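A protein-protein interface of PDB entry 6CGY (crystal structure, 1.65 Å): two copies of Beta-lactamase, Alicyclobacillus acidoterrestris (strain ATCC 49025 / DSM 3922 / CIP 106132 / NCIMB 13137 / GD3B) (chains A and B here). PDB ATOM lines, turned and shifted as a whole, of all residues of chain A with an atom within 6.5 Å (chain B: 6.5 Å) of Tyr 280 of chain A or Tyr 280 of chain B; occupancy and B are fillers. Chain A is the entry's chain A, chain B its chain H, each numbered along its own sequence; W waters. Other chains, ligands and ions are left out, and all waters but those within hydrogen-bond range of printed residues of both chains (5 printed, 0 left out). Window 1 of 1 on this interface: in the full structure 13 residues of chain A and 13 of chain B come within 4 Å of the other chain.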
ATOM      1  N   LYS A  10      17.271 -26.909  -0.741  1.00  0.00           N
ATOM      2  CA  LYS A  10      17.596 -26.166  -1.941  1.00  0.00           C
ATOM      3  C   LYS A  10      19.015 -25.628  -1.741  1.00  0.00           C
ATOM      4  O   LYS A  10      19.297 -25.011  -0.723  1.00  0.00           O
ATOM      5  CB  LYS A  10      16.617 -25.004  -2.151  1.00  0.00           C
ATOM      6  CG  LYS A  10      15.214 -25.397  -2.646  1.00  0.00           C
ATOM      7  CD  LYS A  10      14.377 -24.135  -2.863  1.00  0.00           C
ATOM      8  CE  LYS A  10      13.078 -24.372  -3.621  1.00  0.00           C
ATOM      9  NZ  LYS A  10      12.256 -25.417  -2.969  1.00  0.00           N
ATOM     10  N   LEU A  11      19.887 -25.851  -2.726  1.00  0.00           N
ATOM     11  CA  LEU A  11      21.275 -25.379  -2.670  1.00  0.00           C
ATOM     12  C   LEU A  11      21.493 -24.220  -3.660  1.00  0.00           C
ATOM     13  O   LEU A  11      21.113 -24.316  -4.830  1.00  0.00           O
ATOM     14  CB  LEU A  11      22.224 -26.543  -2.957  1.00  0.00           C
ATOM     15  CG  LEU A  11      23.742 -26.286  -2.963  1.00  0.00           C
ATOM     16  CD1 LEU A  11      24.498 -27.575  -2.679  1.00  0.00           C
ATOM     17  CD2 LEU A  11      24.166 -25.699  -4.294  1.00  0.00           C
ATOM     18  N   TYR A  12      22.097 -23.138  -3.173  1.00  0.00           N
ATOM     19  CA  TYR A  12      22.303 -21.924  -3.932  1.00  0.00           C
ATOM     20  C   TYR A  12      23.793 -21.647  -4.096  1.00  0.00           C
ATOM     21  O   TYR A  12      24.549 -21.741  -3.135  1.00  0.00           O
ATOM     22  CB  TYR A  12      21.713 -20.706  -3.217  1.00  0.00           C
ATOM     23  CG  TYR A  12      20.231 -20.744  -2.986  1.00  0.00           C
ATOM     24  CD1 TYR A  12      19.691 -21.519  -1.979  1.00  0.00           C
ATOM     25  CD2 TYR A  12      19.367 -19.992  -3.781  1.00  0.00           C
ATOM     26  CE1 TYR A  12      18.324 -21.562  -1.758  1.00  0.00           C
ATOM     27  CE2 TYR A  12      17.999 -20.023  -3.561  1.00  0.00           C
ATOM     28  CZ  TYR A  12      17.489 -20.814  -2.556  1.00  0.00           C
ATOM     29  OH  TYR A  12      16.132 -20.862  -2.323  1.00  0.00           O
ATOM     30  N   VAL A  13      24.191 -21.258  -5.299  1.00  0.00           N
ATOM     31  CA  VAL A  13      25.539 -20.791  -5.580  1.00  0.00           C
ATOM     32  C   VAL A  13      25.486 -19.273  -5.658  1.00  0.00           C
ATOM     33  O   VAL A  13      24.802 -18.707  -6.520  1.00  0.00           O
ATOM     34  CB  VAL A  13      26.085 -21.364  -6.899  1.00  0.00           C
ATOM     35  CG1 VAL A  13      27.445 -20.771  -7.256  1.00  0.00           C
ATOM     36  CG2 VAL A  13      26.145 -22.877  -6.848  1.00  0.00           C
ATOM     37  N   GLN A 102      18.815 -10.933  -0.917  1.00  0.00           N
ATOM     38  CA  GLN A 102      17.985 -11.142  -2.101  1.00  0.00           C
ATOM     39  C   GLN A 102      17.345 -12.513  -2.113  1.00  0.00           C
ATOM     40  O   GLN A 102      16.451 -12.776  -2.902  1.00  0.00           O
ATOM     41  CB  GLN A 102      18.768 -10.869  -3.383  1.00  0.00           C
ATOM     42  CG  GLN A 102      19.041  -9.389  -3.582  1.00  0.00           C
ATOM     43  CD  GLN A 102      17.791  -8.517  -3.390  1.00  0.00           C
ATOM     44  OE1 GLN A 102      17.790  -7.560  -2.603  1.00  0.00           O
ATOM     45  NE2 GLN A 102      16.719  -8.854  -4.097  1.00  0.00           N
ATOM     46  N   LEU A 103      17.781 -13.384  -1.215  1.00  0.00           N
ATOM     47  CA  LEU A 103      17.140 -14.663  -1.003  1.00  0.00           C
ATOM     48  C   LEU A 103      16.262 -14.628   0.253  1.00  0.00           C
ATOM     49  O   LEU A 103      15.748 -15.654   0.676  1.00  0.00           O
ATOM     50  CB  LEU A 103      18.199 -15.758  -0.853  1.00  0.00           C
ATOM     51  CG  LEU A 103      19.115 -15.999  -2.047  1.00  0.00           C
ATOM     52  CD1 LEU A 103      20.135 -17.094  -1.762  1.00  0.00           C
ATOM     53  CD2 LEU A 103      18.322 -16.368  -3.279  1.00  0.00           C
ATOM     54  N   ARG A 274      24.230 -22.905 -12.081  1.00  0.00           N
ATOM     55  CA  ARG A 274      23.065 -22.073 -11.929  1.00  0.00           C
ATOM     56  C   ARG A 274      23.273 -21.250 -10.677  1.00  0.00           C
ATOM     57  O   ARG A 274      23.457 -21.819  -9.606  1.00  0.00           O
ATOM     58  CB  ARG A 274      21.810 -22.934 -11.821  1.00  0.00           C
ATOM     59  CG  ARG A 274      20.545 -22.094 -11.717  1.00  0.00           C
ATOM     60  CD  ARG A 274      19.316 -22.861 -12.217  1.00  0.00           C
ATOM     61  NE  ARG A 274      19.124 -24.077 -11.459  1.00  0.00           N
ATOM     62  CZ  ARG A 274      19.318 -25.304 -11.920  1.00  0.00           C
ATOM     63  NH1 ARG A 274      19.712 -25.507 -13.169  1.00  0.00           N
ATOM     64  NH2 ARG A 274      19.112 -26.329 -11.121  1.00  0.00           N
ATOM     65  N   LYS A 275      23.263 -19.924 -10.812  1.00  0.00           N
ATOM     66  CA  LYS A 275      23.521 -19.020  -9.694  1.00  0.00           C
ATOM     67  C   LYS A 275      22.236 -18.588  -8.985  1.00  0.00           C
ATOM     68  O   LYS A 275      21.136 -18.806  -9.491  1.00  0.00           O
ATOM     69  CB  LYS A 275      24.218 -17.750 -10.166  1.00  0.00           C
ATOM     70  CG  LYS A 275      25.208 -17.921 -11.284  1.00  0.00           C
ATOM     71  CD  LYS A 275      26.455 -18.652 -10.839  1.00  0.00           C
ATOM     72  CE  LYS A 275      27.501 -18.553 -11.941  1.00  0.00           C
ATOM     73  NZ  LYS A 275      27.058 -19.080 -13.269  1.00  0.00           N
ATOM     74  N   SER A 276      22.394 -17.916  -7.842  1.00  0.00           N
ATOM     75  CA  SER A 276      21.264 -17.586  -6.968  1.00  0.00           C
ATOM     76  C   SER A 276      20.322 -16.536  -7.565  1.00  0.00           C
ATOM     77  O   SER A 276      19.200 -16.343  -7.086  1.00  0.00           O
ATOM     78  CB  SER A 276      21.763 -17.084  -5.612  1.00  0.00           C
ATOM     79  OG  SER A 276      22.433 -15.837  -5.713  1.00  0.00           O
ATOM     80  N   THR A 277      20.801 -15.842  -8.578  1.00  0.00           N
ATOM     81  CA  THR A 277      19.980 -14.899  -9.328  1.00  0.00           C
ATOM     82  C   THR A 277      19.038 -15.616 -10.294  1.00  0.00           C
ATOM     83  O   THR A 277      18.123 -14.990 -10.853  1.00  0.00           O
ATOM     84  CB  THR A 277      20.861 -13.911 -10.102  1.00  0.00           C
ATOM     85  OG1 THR A 277      21.889 -14.627 -10.811  1.00  0.00           O
ATOM     86  CG2 THR A 277      21.474 -12.868  -9.130  1.00  0.00           C
ATOM     87  N   GLU A 278      19.277 -16.908 -10.514  1.00  0.00           N
ATOM     88  CA  GLU A 278      18.474 -17.714 -11.430  1.00  0.00           C
ATOM     89  C   GLU A 278      17.780 -18.889 -10.750  1.00  0.00           C
ATOM     90  O   GLU A 278      16.764 -19.367 -11.220  1.00  0.00           O
ATOM     91  CB  GLU A 278      19.324 -18.247 -12.599  1.00  0.00           C
ATOM     92  CG  GLU A 278      19.633 -17.232 -13.701  1.00  0.00           C
ATOM     93  CD  GLU A 278      20.774 -16.284 -13.356  1.00  0.00           C
ATOM     94  OE1 GLU A 278      20.624 -15.059 -13.565  1.00  0.00           O
ATOM     95  OE2 GLU A 278      21.826 -16.758 -12.880  1.00  0.00           O
ATOM     96  N   GLY A 279      18.310 -19.371  -9.632  1.00  0.00           N
ATOM     97  CA  GLY A 279      17.688 -20.497  -8.991  1.00  0.00           C
ATOM     98  C   GLY A 279      18.604 -21.241  -8.050  1.00  0.00           C
ATOM     99  O   GLY A 279      19.467 -20.642  -7.404  1.00  0.00           O
ATOM    100  N   TYR A 280      18.418 -22.549  -8.027  1.00  0.00           N
ATOM    101  CA  TYR A 280      18.939 -23.413  -6.993  1.00  0.00           C
ATOM    102  C   TYR A 280      18.977 -24.843  -7.507  1.00  0.00           C
ATOM    103  O   TYR A 280      18.401 -25.182  -8.561  1.00  0.00           O
ATOM    104  CB  TYR A 280      18.048 -23.329  -5.740  1.00  0.00           C
ATOM    105  CG  TYR A 280      16.571 -23.187  -6.049  1.00  0.00           C
ATOM    106  CD1 TYR A 280      15.835 -24.246  -6.575  1.00  0.00           C
ATOM    107  CD2 TYR A 280      15.918 -21.981  -5.826  1.00  0.00           C
ATOM    108  CE1 TYR A 280      14.478 -24.100  -6.880  1.00  0.00           C
ATOM    109  CE2 TYR A 280      14.567 -21.822  -6.121  1.00  0.00           C
ATOM    110  CZ  TYR A 280      13.850 -22.869  -6.651  1.00  0.00           C
ATOM    111  OH  TYR A 280      12.495 -22.680  -6.939  1.00  0.00           O
ATOM    112  N   TYR A 281      19.677 -25.691  -6.773  1.00  0.00           N
ATOM    113  CA  TYR A 281      19.699 -27.116  -7.040  1.00  0.00           C
ATOM    114  C   TYR A 281      18.901 -27.847  -5.966  1.00  0.00           C
ATOM    115  O   TYR A 281      19.034 -27.562  -4.766  1.00  0.00           O
ATOM    116  CB  TYR A 281      21.135 -27.646  -7.011  1.00  0.00           C
ATOM    117  CG  TYR A 281      22.014 -27.142  -8.130  1.00  0.00           C
ATOM    118  CD1 TYR A 281      22.664 -25.921  -8.019  1.00  0.00           C
ATOM    119  CD2 TYR A 281      22.149 -27.855  -9.323  1.00  0.00           C
ATOM    120  CE1 TYR A 281      23.454 -25.440  -9.041  1.00  0.00           C
ATOM    121  CE2 TYR A 281      22.957 -27.387 -10.347  1.00  0.00           C
ATOM    122  CZ  TYR A 281      23.601 -26.173 -10.198  1.00  0.00           C
ATOM    123  OH  TYR A 281      24.382 -25.668 -11.209  1.00  0.00           O
ATOM    124  N   GLU A 282      18.050 -28.765  -6.409  1.00  0.00           N
ATOM    125  CA  GLU A 282      17.246 -29.594  -5.515  1.00  0.00           C
ATOM    126  C   GLU A 282      17.729 -31.038  -5.596  1.00  0.00           C
ATOM    127  O   GLU A 282      17.257 -31.906  -4.853  1.00  0.00           O
ATOM    128  CB  GLU A 282      15.754 -29.512  -5.883  1.00  0.00           C
ATOM    129  CG  GLU A 282      15.162 -28.107  -5.826  1.00  0.00           C
ATOM    130  CD  GLU A 282      13.645 -28.079  -5.999  1.00  0.00           C
ATOM    131  OE1 GLU A 282      13.057 -29.071  -6.496  1.00  0.00           O
ATOM    132  OE2 GLU A 282      13.033 -27.044  -5.645  1.00  0.00           O
ATOM    133  N   LYS B  10      10.410 -12.158  -7.913  1.00  0.00           N
ATOM    134  CA  LYS B  10      10.819 -13.410  -8.568  1.00  0.00           C
ATOM    135  C   LYS B  10       9.599 -14.060  -9.223  1.00  0.00           C
ATOM    136  O   LYS B  10       8.561 -14.202  -8.587  1.00  0.00           O
ATOM    137  CB  LYS B  10      11.428 -14.392  -7.568  1.00  0.00           C
ATOM    138  CG  LYS B  10      12.806 -14.014  -7.022  1.00  0.00           C
ATOM    139  CD  LYS B  10      13.237 -15.027  -5.973  1.00  0.00           C
ATOM    140  CE  LYS B  10      14.654 -14.802  -5.446  1.00  0.00           C
ATOM    141  NZ  LYS B  10      14.876 -13.419  -4.953  1.00  0.00           N
ATOM    142  N   LEU B  11       9.747 -14.474 -10.477  1.00  0.00           N
ATOM    143  CA  LEU B  11       8.672 -15.131 -11.226  1.00  0.00           C
ATOM    144  C   LEU B  11       8.962 -16.618 -11.368  1.00  0.00           C
ATOM    145  O   LEU B  11      10.076 -17.000 -11.760  1.00  0.00           O
ATOM    146  CB  LEU B  11       8.522 -14.496 -12.603  1.00  0.00           C
ATOM    147  CG  LEU B  11       7.403 -15.011 -13.516  1.00  0.00           C
ATOM    148  CD1 LEU B  11       6.889 -13.895 -14.404  1.00  0.00           C
ATOM    149  CD2 LEU B  11       7.874 -16.191 -14.356  1.00  0.00           C
ATOM    150  N   TYR B  12       7.973 -17.435 -11.016  1.00  0.00           N
ATOM    151  CA  TYR B  12       8.093 -18.883 -11.098  1.00  0.00           C
ATOM    152  C   TYR B  12       7.127 -19.481 -12.111  1.00  0.00           C
ATOM    153  O   TYR B  12       5.954 -19.100 -12.146  1.00  0.00           O
ATOM    154  CB  TYR B  12       7.798 -19.550  -9.763  1.00  0.00           C
ATOM    155  CG  TYR B  12       8.659 -19.131  -8.586  1.00  0.00           C
ATOM    156  CD1 TYR B  12       8.406 -17.961  -7.913  1.00  0.00           C
ATOM    157  CD2 TYR B  12       9.727 -19.930  -8.146  1.00  0.00           C
ATOM    158  CE1 TYR B  12       9.167 -17.581  -6.828  1.00  0.00           C
ATOM    159  CE2 TYR B  12      10.497 -19.552  -7.069  1.00  0.00           C
ATOM    160  CZ  TYR B  12      10.210 -18.376  -6.415  1.00  0.00           C
ATOM    161  OH  TYR B  12      10.961 -17.967  -5.326  1.00  0.00           O
ATOM    162  N   VAL B  13       7.614 -20.467 -12.870  1.00  0.00           N
ATOM    163  CA  VAL B  13       6.789 -21.289 -13.744  1.00  0.00           C
ATOM    164  C   VAL B  13       6.569 -22.632 -13.095  1.00  0.00           C
ATOM    165  O   VAL B  13       7.533 -23.373 -12.820  1.00  0.00           O
ATOM    166  CB  VAL B  13       7.464 -21.479 -15.120  1.00  0.00           C
ATOM    167  CG1 VAL B  13       6.663 -22.414 -16.014  1.00  0.00           C
ATOM    168  CG2 VAL B  13       7.717 -20.131 -15.790  1.00  0.00           C
ATOM    169  N   GLN B 102       6.088 -26.565  -2.060  1.00  0.00           N
ATOM    170  CA  GLN B 102       7.530 -26.739  -2.258  1.00  0.00           C
ATOM    171  C   GLN B 102       8.282 -25.423  -2.386  1.00  0.00           C
ATOM    172  O   GLN B 102       9.492 -25.385  -2.212  1.00  0.00           O
ATOM    173  CB  GLN B 102       7.824 -27.644  -3.454  1.00  0.00           C
ATOM    174  CG  GLN B 102       7.521 -29.108  -3.179  1.00  0.00           C
ATOM    175  CD  GLN B 102       8.129 -29.599  -1.865  1.00  0.00           C
ATOM    176  OE1 GLN B 102       7.410 -30.012  -0.950  1.00  0.00           O
ATOM    177  NE2 GLN B 102       9.456 -29.541  -1.762  1.00  0.00           N
ATOM    178  N   LEU B 103       7.566 -24.338  -2.688  1.00  0.00           N
ATOM    179  CA  LEU B 103       8.148 -22.996  -2.656  1.00  0.00           C
ATOM    180  C   LEU B 103       7.893 -22.274  -1.315  1.00  0.00           C
ATOM    181  O   LEU B 103       8.276 -21.124  -1.155  1.00  0.00           O
ATOM    182  CB  LEU B 103       7.565 -22.152  -3.785  1.00  0.00           C
ATOM    183  CG  LEU B 103       7.833 -22.644  -5.205  1.00  0.00           C
ATOM    184  CD1 LEU B 103       7.112 -21.758  -6.201  1.00  0.00           C
ATOM    185  CD2 LEU B 103       9.324 -22.669  -5.497  1.00  0.00           C
ATOM    186  N   ARG B 274      12.687 -22.164 -17.332  1.00  0.00           N
ATOM    187  CA  ARG B 274      13.184 -22.597 -16.041  1.00  0.00           C
ATOM    188  C   ARG B 274      11.973 -22.773 -15.114  1.00  0.00           C
ATOM    189  O   ARG B 274      11.233 -21.828 -14.865  1.00  0.00           O
ATOM    190  CB  ARG B 274      14.151 -21.532 -15.506  1.00  0.00           C
ATOM    191  CG  ARG B 274      14.799 -21.885 -14.186  1.00  0.00           C
ATOM    192  CD  ARG B 274      16.128 -21.163 -14.029  1.00  0.00           C
ATOM    193  NE  ARG B 274      15.991 -19.706 -14.031  1.00  0.00           N
ATOM    194  CZ  ARG B 274      16.398 -18.909 -15.009  1.00  0.00           C
ATOM    195  NH1 ARG B 274      16.229 -17.597 -14.913  1.00  0.00           N
ATOM    196  NH2 ARG B 274      16.992 -19.415 -16.078  1.00  0.00           N
ATOM    197  N   LYS B 275      11.762 -23.989 -14.637  1.00  0.00           N
ATOM    198  CA  LYS B 275      10.598 -24.331 -13.840  1.00  0.00           C
ATOM    199  C   LYS B 275      10.916 -24.159 -12.361  1.00  0.00           C
ATOM    200  O   LYS B 275      12.069 -23.976 -11.974  1.00  0.00           O
ATOM    201  CB  LYS B 275      10.142 -25.764 -14.138  1.00  0.00           C
ATOM    202  CG  LYS B 275       9.039 -25.845 -15.201  1.00  0.00           C
ATOM    203  CD  LYS B 275       9.526 -25.500 -16.593  1.00  0.00           C
ATOM    204  CE  LYS B 275       9.873 -26.755 -17.373  1.00  0.00           C
ATOM    205  NZ  LYS B 275      10.946 -26.531 -18.371  1.00  0.00           N
ATOM    206  N   SER B 276       9.879 -24.228 -11.542  1.00  0.00           N
ATOM    207  CA  SER B 276       9.994 -23.914 -10.115  1.00  0.00           C
ATOM    208  C   SER B 276      10.839 -24.917  -9.325  1.00  0.00           C
ATOM    209  O   SER B 276      11.203 -24.643  -8.197  1.00  0.00           O
ATOM    210  CB  SER B 276       8.603 -23.792  -9.474  1.00  0.00           C
ATOM    211  OG  SER B 276       7.923 -25.030  -9.415  1.00  0.00           O
ATOM    212  N   THR B 277      11.102 -26.082  -9.905  1.00  0.00           N
ATOM    213  CA  THR B 277      12.020 -27.053  -9.308  1.00  0.00           C
ATOM    214  C   THR B 277      13.483 -26.670  -9.517  1.00  0.00           C
ATOM    215  O   THR B 277      14.370 -27.248  -8.867  1.00  0.00           O
ATOM    216  CB  THR B 277      11.763 -28.451  -9.892  1.00  0.00           C
ATOM    217  OG1 THR B 277      11.649 -28.343 -11.314  1.00  0.00           O
ATOM    218  CG2 THR B 277      10.491 -29.025  -9.322  1.00  0.00           C
ATOM    219  N   GLU B 278      13.741 -25.691 -10.383  1.00  0.00           N
ATOM    220  CA  GLU B 278      15.103 -25.235 -10.706  1.00  0.00           C
ATOM    221  C   GLU B 278      15.363 -23.771 -10.367  1.00  0.00           C
ATOM    222  O   GLU B 278      16.511 -23.368 -10.153  1.00  0.00           O
ATOM    223  CB  GLU B 278      15.411 -25.455 -12.192  1.00  0.00           C
ATOM    224  CG  GLU B 278      15.862 -26.870 -12.545  1.00  0.00           C
ATOM    225  CD  GLU B 278      14.712 -27.850 -12.725  1.00  0.00           C
ATOM    226  OE1 GLU B 278      14.805 -28.985 -12.208  1.00  0.00           O
ATOM    227  OE2 GLU B 278      13.722 -27.499 -13.402  1.00  0.00           O
ATOM    228  N   GLY B 279      14.319 -22.952 -10.338  1.00  0.00           N
ATOM    229  CA  GLY B 279      14.508 -21.565 -10.002  1.00  0.00           C
ATOM    230  C   GLY B 279      13.393 -20.682 -10.505  1.00  0.00           C
ATOM    231  O   GLY B 279      12.232 -21.059 -10.451  1.00  0.00           O
ATOM    232  N   TYR B 280      13.783 -19.514 -10.990  1.00  0.00           N
ATOM    233  CA  TYR B 280      12.880 -18.384 -11.157  1.00  0.00           C
ATOM    234  C   TYR B 280      13.493 -17.357 -12.087  1.00  0.00           C
ATOM    235  O   TYR B 280      14.662 -17.426 -12.450  1.00  0.00           O
ATOM    236  CB  TYR B 280      12.583 -17.719  -9.801  1.00  0.00           C
ATOM    237  CG  TYR B 280      13.784 -17.698  -8.856  1.00  0.00           C
ATOM    238  CD1 TYR B 280      14.867 -16.859  -9.096  1.00  0.00           C
ATOM    239  CD2 TYR B 280      13.841 -18.543  -7.763  1.00  0.00           C
ATOM    240  CE1 TYR B 280      15.976 -16.850  -8.260  1.00  0.00           C
ATOM    241  CE2 TYR B 280      14.941 -18.537  -6.918  1.00  0.00           C
ATOM    242  CZ  TYR B 280      16.007 -17.696  -7.180  1.00  0.00           C
ATOM    243  OH  TYR B 280      17.106 -17.687  -6.332  1.00  0.00           O
ATOM    244  N   TYR B 281      12.688 -16.376 -12.466  1.00  0.00           N
ATOM    245  CA  TYR B 281      13.154 -15.294 -13.278  1.00  0.00           C
ATOM    246  C   TYR B 281      13.163 -14.033 -12.427  1.00  0.00           C
ATOM    247  O   TYR B 281      12.197 -13.750 -11.708  1.00  0.00           O
ATOM    248  CB  TYR B 281      12.234 -15.112 -14.501  1.00  0.00           C
ATOM    249  CG  TYR B 281      12.316 -16.251 -15.485  1.00  0.00           C
ATOM    250  CD1 TYR B 281      11.582 -17.398 -15.299  1.00  0.00           C
ATOM    251  CD2 TYR B 281      13.139 -16.178 -16.610  1.00  0.00           C
ATOM    252  CE1 TYR B 281      11.658 -18.453 -16.187  1.00  0.00           C
ATOM    253  CE2 TYR B 281      13.225 -17.230 -17.499  1.00  0.00           C
ATOM    254  CZ  TYR B 281      12.472 -18.370 -17.280  1.00  0.00           C
ATOM    255  OH  TYR B 281      12.533 -19.455 -18.148  1.00  0.00           O
ATOM    256  N   GLU B 282      14.253 -13.275 -12.506  1.00  0.00           N
ATOM    257  CA  GLU B 282      14.349 -11.986 -11.819  1.00  0.00           C
ATOM    258  C   GLU B 282      14.442 -10.846 -12.834  1.00  0.00           C
ATOM    259  O   GLU B 282      14.489  -9.670 -12.462  1.00  0.00           O
ATOM    260  CB  GLU B 282      15.566 -11.961 -10.874  1.00  0.00           C
ATOM    261  CG  GLU B 282      15.424 -12.867  -9.657  1.00  0.00           C
ATOM    262  CD  GLU B 282      16.646 -12.869  -8.751  1.00  0.00           C
ATOM    263  OE1 GLU B 282      17.557 -12.031  -8.933  1.00  0.00           O
ATOM    264  OE2 GLU B 282      16.690 -13.725  -7.844  1.00  0.00           O
HETATM  265  O   HOH W   1      16.953  -9.637  -6.809  1.00  0.00           O
HETATM  266  O   HOH W   2      18.514 -13.736  -5.788  1.00  0.00           O
HETATM  267  O   HOH W   3      16.956 -28.042  -9.127  1.00  0.00           O
HETATM  268  O   HOH W   4      16.769 -14.735 -13.242  1.00  0.00           O
HETATM  269  O   HOH W   5      10.475 -26.000  -5.805  1.00  0.00           O
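Of the 15 printed residues of chain B, 11 touch a printed residue of chain A. Hydrophobic or aromatic side chains of chain B within 4 Å of the printed part of chain A: Tyr 12, Leu 103 and Tyr 280. Of the 15 printed residues of chain A, 11 touch a printed residue of chain B. Printed residues of chain A that touch a printed residue of chain B: Lys 10, Tyr 12, Gln 102, Leu 103, Arg 274, Ser 276, Thr 277, Glu 278, Gly 279, Tyr 280 and Glu 282. Hydrophobic or aromatic side chains of chain A that line the printed part of chain B: Tyr 12, Leu 103 and Tyr 280. Along chain A the printed residues that touch a printed residue of chain B span positions 10 to 282. Among the printed residues, no Asp or Glu carboxylate lies within 4 Å of a Lys or Arg side-chain nitrogen of the other chain.
Tyr 12 of chain A touches Tyr 280 of chain B, and with the chains exchanged Tyr 280 of chain A touches Tyr 12 of chain B. Thr 277 of chain A touches Tyr 280 of chain B, and with the chains exchanged Tyr 280 of chain A touches Thr 277 of chain B. Glu 278 of chain A touches Tyr 280 of chain B, and with the chains exchanged Tyr 280 of chain A touches Glu 278 of chain B. Tyr 280 of chain A touches its own counterpart, Tyr 280 of chain B. 15 positions are printed for both chains. Of the 24 pairs that touch across the chains among the printed residues, 24 have their exchanged pair printed and touching as well.
Water W3 lies within hydrogen-bond range of the backbone carbonyl oxygen of Thr 277 of chain B, the backbone NH of Glu 282 of chain A, the backbone carbonyl oxygen of Tyr 280 of chain A and the guanidinium group of Arg 274 of chain A. Water W2 bridges the side-chain carboxylate (OE2) of Glu 282 of chain B (2.7 Å) and the backbone carbonyl oxygen (O) of Ser 276 of chain A (3.0 Å). Water W4 lies within hydrogen-bond range of the backbone carbonyl oxygen (O) of Thr 277 of chain A, the backbone NH (N) of Glu 282 of chain B and the guanidinium group (NH1) of Arg 274 of chain B. Water W5 lies within hydrogen-bond range of OE2 of Glu 282 of chain A (2.8 Å), O of Ser 276 of chain B (2.8 Å) and NZ of Lys 10 of chain A (3.4 Å). Water W1 lies within hydrogen-bond range of NE2 of Gln 102 of chain A (2.8 Å) and OE1 of Glu 282 of chain B (3.3 Å).
NZ of Lys 10 of chain A is in salt-bridge range of OE2 of Glu 282 of chain A, 3.2 Å away. O of Val 13 of chain A lies within hydrogen-bond range of N of Ser 276 of chain A, at 2.9 Å. The guanidinium group (NH2) of Arg 274 of chain A lies within hydrogen-bond range of the backbone carbonyl oxygen (O) of Tyr 280 of chain A. The backbone NH (N) of Arg 274 of chain A lies within hydrogen-bond range of the side-chain hydroxyl (OH) of Tyr 281 of chain A. OE2 of Glu 282 of chain B lies within salt-bridge range of NZ of Lys 10 of chain B, 3.4 Å away. The backbone NH of Ser 276 of chain B sits at hydrogen-bond distance from the backbone carbonyl oxygen of Val 13 of chain B (2.8 Å).
The backbone carbonyl oxygen of Gln 102 of chain B is in hydrogen-bond range of the side-chain amino group of Lys 10 of chain A. The side-chain amino group (NZ) of Lys 10 of chain B sits at hydrogen-bond distance from the backbone carbonyl oxygen (O) of Gln 102 of chain A, 2.7 Å away. NE of Arg 274 of chain A lies within hydrogen-bond range of O of Glu 278 of chain B (3.0 Å). The side-chain hydroxyl of Tyr 280 of chain B lies within hydrogen-bond range of the backbone carbonyl oxygen of Ser 276 of chain A (2.6 Å). The guanidinium group (NE) of Arg 274 of chain B is in hydrogen-bond range of the backbone carbonyl oxygen (O) of Glu 278 of chain A (2.9 Å). The backbone NH (N) of Tyr 280 of chain B lies within hydrogen-bond range of the backbone carbonyl oxygen (O) of Glu 278 of chain A (3.0 Å). The side-chain hydroxyl (OH) of Tyr 280 of chain A sits at hydrogen-bond distance from the backbone carbonyl oxygen (O) of Ser 276 of chain B (2.7 Å). The backbone NH of Tyr 280 of chain A lies within hydrogen-bond range of the backbone carbonyl oxygen of Glu 278 of chain B. The side-chain carboxylate of Glu 282 of chain A lies close to the backbone carbonyl oxygen of Thr 277 of chain B (3.3 Å).
Of the printed residues of chain B, Leu 103 of chain A touches Tyr 280. Of the printed residues of chain B, Tyr 280 of chain A touches Tyr 12, Leu 103, Ser 276, Thr 277, Glu 278, Gly 279 and Tyr 280. Tyr 281 of chain A touches none of the printed residues of chain B. Val 13 of chain B touches none of the printed residues of chain A. Of the printed residues of chain A, Thr 277 of chain B touches Tyr 280 and Glu 282. Printed residues of chain A within 4 Å of Gly 279 of chain B: Glu 278, Gly 279 and Tyr 280. Tyr 280 of chain B touches just these residues of chain A: Tyr 12, Leu 103, Ser 276, Thr 277, Glu 278, Gly 279 and Tyr 280. Printed residues of chain A within 4 Å of Glu 282 of chain B: Ser 276 and Thr 277.
Among the printed residues, merely in contact across the chains: Tyr 12 of chain A with Tyr 280 of chain B, Leu 103 of chain A with Tyr 280 of chain B, Ser 276 of chain A with Glu 282 of chain B, Thr 277 of chain A with Tyr 280 of chain B, Thr 277 of chain A with Glu 282 of chain B, Glu 278 of chain A with Gly 279 of chain B, Gly 279 of chain A with Glu 278 of chain B, Gly 279 of chain A with Gly 279 of chain B, Gly 279 of chain A with Tyr 280 of chain B, Tyr 280 of chain A with Tyr 12 of chain B, Tyr 280 of chain A with Leu 103 of chain B, Tyr 280 of chain A with Thr 277 of chain B, Tyr 280 of chain A with Gly 279 of chain B, Tyr 280 of chain A with Tyr 280 of chain B and Glu 282 of chain A with Ser 276 of chain B.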
